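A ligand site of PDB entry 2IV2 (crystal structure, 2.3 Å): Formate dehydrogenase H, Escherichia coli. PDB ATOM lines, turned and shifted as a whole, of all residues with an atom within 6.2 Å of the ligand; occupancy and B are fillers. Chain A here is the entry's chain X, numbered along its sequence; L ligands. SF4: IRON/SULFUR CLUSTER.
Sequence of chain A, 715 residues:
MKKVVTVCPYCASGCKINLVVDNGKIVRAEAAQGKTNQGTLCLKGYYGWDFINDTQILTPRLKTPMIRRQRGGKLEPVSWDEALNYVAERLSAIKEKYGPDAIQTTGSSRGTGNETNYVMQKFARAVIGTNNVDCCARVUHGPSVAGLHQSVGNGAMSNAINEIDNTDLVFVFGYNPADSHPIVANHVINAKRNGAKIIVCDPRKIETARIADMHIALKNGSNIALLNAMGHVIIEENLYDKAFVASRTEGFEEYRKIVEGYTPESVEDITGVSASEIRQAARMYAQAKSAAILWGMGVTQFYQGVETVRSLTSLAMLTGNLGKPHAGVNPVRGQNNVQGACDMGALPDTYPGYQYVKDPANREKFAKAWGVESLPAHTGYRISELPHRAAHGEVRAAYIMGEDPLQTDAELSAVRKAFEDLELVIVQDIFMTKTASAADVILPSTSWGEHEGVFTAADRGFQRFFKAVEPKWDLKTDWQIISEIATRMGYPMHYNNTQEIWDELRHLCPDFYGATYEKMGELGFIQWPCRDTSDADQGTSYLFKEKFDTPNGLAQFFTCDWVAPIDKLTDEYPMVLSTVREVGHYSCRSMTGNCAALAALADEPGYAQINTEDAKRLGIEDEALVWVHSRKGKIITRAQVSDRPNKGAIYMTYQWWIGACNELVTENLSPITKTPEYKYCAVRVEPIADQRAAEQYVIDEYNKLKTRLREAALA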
ATOM      1  N   CYS A   8      -7.537  30.828 -16.849  1.00  0.00           N
ATOM      2  CA  CYS A   8      -8.563  31.569 -17.561  1.00  0.00           C
ATOM      3  C   CYS A   8      -9.469  32.383 -16.626  1.00  0.00           C
ATOM      4  O   CYS A   8      -9.918  31.862 -15.606  1.00  0.00           O
ATOM      5  CB  CYS A   8      -9.434  30.626 -18.372  1.00  0.00           C
ATOM      6  SG  CYS A   8     -10.548  31.526 -19.475  1.00  0.00           S
ATOM      7  N   PRO A   9      -9.741  33.659 -16.956  1.00  0.00           N
ATOM      8  CA  PRO A   9     -10.584  34.515 -16.128  1.00  0.00           C
ATOM      9  C   PRO A   9     -12.064  34.523 -16.481  1.00  0.00           C
ATOM     10  O   PRO A   9     -12.767  35.424 -16.036  1.00  0.00           O
ATOM     11  CB  PRO A   9     -10.001  35.895 -16.414  1.00  0.00           C
ATOM     12  CG  PRO A   9      -9.645  35.832 -17.814  1.00  0.00           C
ATOM     13  CD  PRO A   9      -9.184  34.420 -18.082  1.00  0.00           C
ATOM     14  N   TYR A  10     -12.535  33.542 -17.239  1.00  0.00           N
ATOM     15  CA  TYR A  10     -13.909  33.501 -17.662  1.00  0.00           C
ATOM     16  C   TYR A  10     -14.708  32.549 -16.793  1.00  0.00           C
ATOM     17  O   TYR A  10     -15.166  32.964 -15.709  1.00  0.00           O
ATOM     18  CB  TYR A  10     -14.002  33.232 -19.173  1.00  0.00           C
ATOM     19  CG  TYR A  10     -13.507  34.446 -19.919  1.00  0.00           C
ATOM     20  CD1 TYR A  10     -14.234  35.628 -19.882  1.00  0.00           C
ATOM     21  CD2 TYR A  10     -12.278  34.451 -20.574  1.00  0.00           C
ATOM     22  CE1 TYR A  10     -13.780  36.781 -20.514  1.00  0.00           C
ATOM     23  CE2 TYR A  10     -11.802  35.595 -21.197  1.00  0.00           C
ATOM     24  CZ  TYR A  10     -12.558  36.756 -21.172  1.00  0.00           C
ATOM     25  OH  TYR A  10     -12.131  37.888 -21.826  1.00  0.00           O
ATOM     26  N   CYS A  11     -14.877  31.302 -17.231  1.00  0.00           N
ATOM     27  CA  CYS A  11     -15.700  30.363 -16.491  1.00  0.00           C
ATOM     28  C   CYS A  11     -14.868  29.526 -15.532  1.00  0.00           C
ATOM     29  O   CYS A  11     -13.633  29.571 -15.527  1.00  0.00           O
ATOM     30  CB  CYS A  11     -16.532  29.495 -17.465  1.00  0.00           C
ATOM     31  SG  CYS A  11     -15.741  28.038 -18.162  1.00  0.00           S
ATOM     32  N   ALA A  12     -15.558  28.735 -14.708  1.00  0.00           N
ATOM     33  CA  ALA A  12     -14.900  28.011 -13.618  1.00  0.00           C
ATOM     34  C   ALA A  12     -14.233  26.697 -14.042  1.00  0.00           C
ATOM     35  O   ALA A  12     -13.815  25.930 -13.171  1.00  0.00           O
ATOM     36  CB  ALA A  12     -15.906  27.755 -12.517  1.00  0.00           C
ATOM     37  N   SER A  13     -14.092  26.442 -15.347  1.00  0.00           N
ATOM     38  CA  SER A  13     -13.390  25.242 -15.839  1.00  0.00           C
ATOM     39  C   SER A  13     -11.917  25.216 -15.428  1.00  0.00           C
ATOM     40  O   SER A  13     -11.304  24.149 -15.376  1.00  0.00           O
ATOM     41  CB  SER A  13     -13.465  25.139 -17.361  1.00  0.00           C
ATOM     42  OG  SER A  13     -14.761  24.888 -17.811  1.00  0.00           O
ATOM     43  N   GLY A  14     -11.340  26.391 -15.224  1.00  0.00           N
ATOM     44  CA  GLY A  14     -10.014  26.516 -14.628  1.00  0.00           C
ATOM     45  C   GLY A  14      -8.849  26.190 -15.543  1.00  0.00           C
ATOM     46  O   GLY A  14      -7.791  25.797 -15.062  1.00  0.00           O
ATOM     47  N   CYS A  15      -9.056  26.369 -16.855  1.00  0.00           N
ATOM     48  CA  CYS A  15      -8.042  26.106 -17.859  1.00  0.00           C
ATOM     49  C   CYS A  15      -6.782  26.926 -17.610  1.00  0.00           C
ATOM     50  O   CYS A  15      -6.852  28.124 -17.351  1.00  0.00           O
ATOM     51  CB  CYS A  15      -8.565  26.450 -19.271  1.00  0.00           C
ATOM     52  SG  CYS A  15     -10.050  25.543 -19.785  1.00  0.00           S
ATOM     53  N   ILE A  17      -3.452  28.652 -19.074  1.00  0.00           N
ATOM     54  CA  ILE A  17      -3.142  29.363 -20.298  1.00  0.00           C
ATOM     55  C   ILE A  17      -1.698  29.831 -20.210  1.00  0.00           C
ATOM     56  O   ILE A  17      -1.278  30.312 -19.167  1.00  0.00           O
ATOM     57  CB  ILE A  17      -4.060  30.586 -20.452  1.00  0.00           C
ATOM     58  CG1 ILE A  17      -5.506  30.123 -20.661  1.00  0.00           C
ATOM     59  CG2 ILE A  17      -3.629  31.457 -21.611  1.00  0.00           C
ATOM     60  CD1 ILE A  17      -6.493  31.267 -20.741  1.00  0.00           C
ATOM     61  N   ASN A  37      -7.818  21.262 -18.454  1.00  0.00           N
ATOM     62  CA  ASN A  37      -7.870  21.549 -19.899  1.00  0.00           C
ATOM     63  C   ASN A  37      -6.881  20.800 -20.779  1.00  0.00           C
ATOM     64  O   ASN A  37      -7.201  20.538 -21.929  1.00  0.00           O
ATOM     65  CB  ASN A  37      -7.777  23.046 -20.164  1.00  0.00           C
ATOM     66  CG  ASN A  37      -6.463  23.618 -19.826  1.00  0.00           C
ATOM     67  OD1 ASN A  37      -5.935  23.347 -18.748  1.00  0.00           O
ATOM     68  ND2 ASN A  37      -5.897  24.416 -20.746  1.00  0.00           N
ATOM     69  N   THR A  40      -6.130  22.465 -24.220  1.00  0.00           N
ATOM     70  CA  THR A  40      -7.283  23.016 -24.921  1.00  0.00           C
ATOM     71  C   THR A  40      -7.832  24.240 -24.220  1.00  0.00           C
ATOM     72  O   THR A  40      -7.766  24.360 -23.008  1.00  0.00           O
ATOM     73  CB  THR A  40      -8.414  21.996 -25.067  1.00  0.00           C
ATOM     74  OG1 THR A  40      -8.943  21.666 -23.779  1.00  0.00           O
ATOM     75  CG2 THR A  40      -7.901  20.747 -25.760  1.00  0.00           C
ATOM     76  N   LEU A  41      -8.379  25.155 -25.028  1.00  0.00           N
ATOM     77  CA  LEU A  41      -9.133  26.291 -24.562  1.00  0.00           C
ATOM     78  C   LEU A  41     -10.310  26.377 -25.470  1.00  0.00           C
ATOM     79  O   LEU A  41     -10.249  25.906 -26.598  1.00  0.00           O
ATOM     80  CB  LEU A  41      -8.348  27.601 -24.732  1.00  0.00           C
ATOM     81  CG  LEU A  41      -7.038  27.721 -23.955  1.00  0.00           C
ATOM     82  CD1 LEU A  41      -6.313  28.985 -24.391  1.00  0.00           C
ATOM     83  CD2 LEU A  41      -7.264  27.651 -22.414  1.00  0.00           C
ATOM     84  N   CYS A  42     -11.371  27.005 -24.995  1.00  0.00           N
ATOM     85  CA  CYS A  42     -12.460  27.422 -25.866  1.00  0.00           C
ATOM     86  C   CYS A  42     -12.062  28.788 -26.469  1.00  0.00           C
ATOM     87  O   CYS A  42     -11.021  29.357 -26.143  1.00  0.00           O
ATOM     88  CB  CYS A  42     -13.786  27.491 -25.087  1.00  0.00           C
ATOM     89  SG  CYS A  42     -13.972  28.923 -23.980  1.00  0.00           S
ATOM     90  N   LEU A  43     -12.890  29.286 -27.389  1.00  0.00           N
ATOM     91  CA  LEU A  43     -12.784  30.651 -27.963  1.00  0.00           C
ATOM     92  C   LEU A  43     -12.373  31.738 -26.978  1.00  0.00           C
ATOM     93  O   LEU A  43     -11.571  32.582 -27.306  1.00  0.00           O
ATOM     94  CB  LEU A  43     -14.170  31.077 -28.469  1.00  0.00           C
ATOM     95  CG  LEU A  43     -14.537  31.222 -29.921  1.00  0.00           C
ATOM     96  CD1 LEU A  43     -13.718  30.378 -30.857  1.00  0.00           C
ATOM     97  CD2 LEU A  43     -16.027  30.873 -30.024  1.00  0.00           C
ATOM     98  N   LYS A  44     -12.965  31.717 -25.792  1.00  0.00           N
ATOM     99  CA  LYS A  44     -12.773  32.787 -24.812  1.00  0.00           C
ATOM    100  C   LYS A  44     -11.381  32.791 -24.162  1.00  0.00           C
ATOM    101  O   LYS A  44     -10.760  33.851 -24.044  1.00  0.00           O
ATOM    102  CB  LYS A  44     -13.886  32.725 -23.754  1.00  0.00           C
ATOM    103  CG  LYS A  44     -15.283  32.917 -24.349  1.00  0.00           C
ATOM    104  CD  LYS A  44     -16.358  33.110 -23.261  1.00  0.00           C
ATOM    105  CE  LYS A  44     -16.554  31.860 -22.398  1.00  0.00           C
ATOM    106  NZ  LYS A  44     -16.766  30.589 -23.170  1.00  0.00           N
ATOM    107  N   GLY A  45     -10.851  31.640 -23.765  1.00  0.00           N
ATOM    108  CA  GLY A  45      -9.473  31.575 -23.305  1.00  0.00           C
ATOM    109  C   GLY A  45      -8.449  31.933 -24.385  1.00  0.00           C
ATOM    110  O   GLY A  45      -7.428  32.568 -24.120  1.00  0.00           O
ATOM    111  N   TYR A  46      -8.739  31.511 -25.605  1.00  0.00           N
ATOM    112  CA  TYR A  46      -7.850  31.656 -26.746  1.00  0.00           C
ATOM    113  C   TYR A  46      -7.784  33.096 -27.229  1.00  0.00           C
ATOM    114  O   TYR A  46      -6.697  33.630 -27.463  1.00  0.00           O
ATOM    115  CB  TYR A  46      -8.341  30.771 -27.886  1.00  0.00           C
ATOM    116  CG  TYR A  46      -7.314  30.484 -28.922  1.00  0.00           C
ATOM    117  CD1 TYR A  46      -6.474  29.395 -28.790  1.00  0.00           C
ATOM    118  CD2 TYR A  46      -7.157  31.304 -30.038  1.00  0.00           C
ATOM    119  CE1 TYR A  46      -5.498  29.129 -29.722  1.00  0.00           C
ATOM    120  CE2 TYR A  46      -6.172  31.042 -30.999  1.00  0.00           C
ATOM    121  CZ  TYR A  46      -5.362  29.947 -30.837  1.00  0.00           C
ATOM    122  OH  TYR A  46      -4.397  29.615 -31.746  1.00  0.00           O
ATOM    123  N   SER A 180     -21.519  26.722 -21.474  1.00  0.00           N
ATOM    124  CA  SER A 180     -21.210  27.246 -20.151  1.00  0.00           C
ATOM    125  C   SER A 180     -19.812  26.948 -19.680  1.00  0.00           C
ATOM    126  O   SER A 180     -19.201  27.768 -19.037  1.00  0.00           O
ATOM    127  CB  SER A 180     -22.164  26.657 -19.102  1.00  0.00           C
ATOM    128  OG  SER A 180     -23.306  27.466 -19.016  1.00  0.00           O
ATOM    129  N   HIS A 181     -19.346  25.730 -19.944  1.00  0.00           N
ATOM    130  CA  HIS A 181     -18.058  25.274 -19.458  1.00  0.00           C
ATOM    131  C   HIS A 181     -17.490  24.330 -20.499  1.00  0.00           C
ATOM    132  O   HIS A 181     -17.460  23.118 -20.284  1.00  0.00           O
ATOM    133  CB  HIS A 181     -18.230  24.535 -18.111  1.00  0.00           C
ATOM    134  CG  HIS A 181     -18.736  25.398 -17.001  1.00  0.00           C
ATOM    135  ND1 HIS A 181     -20.078  25.593 -16.761  1.00  0.00           N
ATOM    136  CD2 HIS A 181     -18.092  26.089 -16.032  1.00  0.00           C
ATOM    137  CE1 HIS A 181     -20.243  26.386 -15.722  1.00  0.00           C
ATOM    138  NE2 HIS A 181     -19.046  26.704 -15.260  1.00  0.00           N
ATOM    139  N   PRO A 182     -17.096  24.862 -21.667  1.00  0.00           N
ATOM    140  CA  PRO A 182     -16.670  23.997 -22.764  1.00  0.00           C
ATOM    141  C   PRO A 182     -15.705  22.904 -22.384  1.00  0.00           C
ATOM    142  O   PRO A 182     -15.832  21.792 -22.878  1.00  0.00           O
ATOM    143  CB  PRO A 182     -16.029  24.983 -23.734  1.00  0.00           C
ATOM    144  CG  PRO A 182     -16.880  26.204 -23.557  1.00  0.00           C
ATOM    145  CD  PRO A 182     -17.066  26.288 -22.070  1.00  0.00           C
ATOM    146  N   ILE A 183     -14.760  23.209 -21.502  1.00  0.00           N
ATOM    147  CA  ILE A 183     -13.768  22.218 -21.101  1.00  0.00           C
ATOM    148  C   ILE A 183     -14.380  21.152 -20.192  1.00  0.00           C
ATOM    149  O   ILE A 183     -14.020  19.994 -20.315  1.00  0.00           O
ATOM    150  CB  ILE A 183     -12.469  22.861 -20.533  1.00  0.00           C
ATOM    151  CG1 ILE A 183     -11.400  22.941 -21.627  1.00  0.00           C
ATOM    152  CG2 ILE A 183     -11.920  22.051 -19.349  1.00  0.00           C
ATOM    153  CD1 ILE A 183     -11.705  23.897 -22.751  1.00  0.00           C
ATOM    154  N   VAL A 184     -15.321  21.533 -19.328  1.00  0.00           N
ATOM    155  CA  VAL A 184     -16.129  20.553 -18.574  1.00  0.00           C
ATOM    156  C   VAL A 184     -16.984  19.703 -19.545  1.00  0.00           C
ATOM    157  O   VAL A 184     -17.106  18.494 -19.345  1.00  0.00           O
ATOM    158  CB  VAL A 184     -17.054  21.219 -17.534  1.00  0.00           C
ATOM    159  CG1 VAL A 184     -17.894  20.177 -16.806  1.00  0.00           C
ATOM    160  CG2 VAL A 184     -16.251  22.007 -16.518  1.00  0.00           C
ATOM    161  N   TYR A 586     -18.914  36.342 -22.632  1.00  0.00           N
ATOM    162  CA  TYR A 586     -19.051  36.198 -21.214  1.00  0.00           C
ATOM    163  C   TYR A 586     -19.970  37.292 -20.667  1.00  0.00           C
ATOM    164  O   TYR A 586     -20.129  38.348 -21.310  1.00  0.00           O
ATOM    165  CB  TYR A 586     -17.696  36.181 -20.516  1.00  0.00           C
ATOM    166  CG  TYR A 586     -17.758  35.442 -19.222  1.00  0.00           C
ATOM    167  CD1 TYR A 586     -17.856  36.131 -18.017  1.00  0.00           C
ATOM    168  CD2 TYR A 586     -17.799  34.051 -19.188  1.00  0.00           C
ATOM    169  CE1 TYR A 586     -17.951  35.470 -16.814  1.00  0.00           C
ATOM    170  CE2 TYR A 586     -17.879  33.359 -17.969  1.00  0.00           C
ATOM    171  CZ  TYR A 586     -17.972  34.083 -16.790  1.00  0.00           C
ATOM    172  OH  TYR A 586     -18.063  33.471 -15.571  1.00  0.00           O
HETATM  173 FE1  SF4 L   1     -13.149  28.365 -22.019  1.00  0.00          FE
HETATM  174 FE2  SF4 L   1     -11.752  29.755 -20.103  1.00  0.00          FE
HETATM  175 FE3  SF4 L   1     -11.555  27.132 -20.207  1.00  0.00          FE
HETATM  176 FE4  SF4 L   1     -13.894  28.327 -19.399  1.00  0.00          FE
HETATM  177  S1  SF4 L   1     -11.864  28.371 -18.333  1.00  0.00           S
HETATM  178  S2  SF4 L   1     -13.653  26.502 -20.878  1.00  0.00           S
HETATM  179  S3  SF4 L   1     -13.962  30.148 -20.697  1.00  0.00           S
HETATM  180  S4  SF4 L   1     -10.795  28.509 -21.909  1.00  0.00           S
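SG of Cys 11 lies close to OG of Ser 13 (3.3 Å).
The backbone carbonyl oxygen of Cys 15 is in hydrogen-bond range of the backbone NH of Cys 8.
The backbone NH (N) of Tyr 10 lies close to the side-chain sulfur (SG) of Cys 8 (3.6 Å).
The side-chain sulfur (SG) of Cys 42 lies close to the side-chain amino group (NZ) of Lys 44, 3.4 Å away.
The backbone carbonyl oxygen (O) of Tyr 10 sits at hydrogen-bond distance from the side-chain hydroxyl (OH) of Tyr 586.
SG of Cys 11 lies close to O of Ser 180 (3.6 Å).
Tyr 10 touches the ligand.
Leu 41 touches the ligand.
Pro 182 touches the ligand.
Hydrophobic or aromatic side chains that line the ligand: Tyr 10, Leu 41, Pro 182 and Ile 183.
Of the 23 residues printed, 12 come within 4 Å of the ligand.
The backbone NH of Gly 14 lies close to a sulfur (S1) of the ligand, at 3.7 Å.
S3 of the ligand sits close to NZ of Lys 44 (3.8 Å).
The side-chain sulfur of Cys 11 is bound to an iron atom (FE4) of the ligand, 2.2 Å away.
The backbone NH (N) of Cys 15 sits close to a sulfur (S1) of the ligand.
A sulfur (S2) of the ligand lies close to the backbone NH (N) of Ile 183 (3.5 Å).
The backbone NH (N) of Gly 45 lies close to a sulfur (S4) of the ligand (3.6 Å).
The side-chain sulfur (SG) of Cys 42 is bound to an iron atom (FE1) of the ligand, 2.2 Å away.
SG of Cys 8 is bound to FE2 of the ligand.
OG of Ser 13 sits close to S2 of the ligand (3.6 Å).
The backbone NH (N) of Cys 42 lies close to a sulfur (S4) of the ligand, at 3.5 Å.
An iron atom (FE3) of the ligand is bound by the side-chain sulfur (SG) of Cys 15.
A sulfur (S3) of the ligand lies close to the backbone NH (N) of Cys 11.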
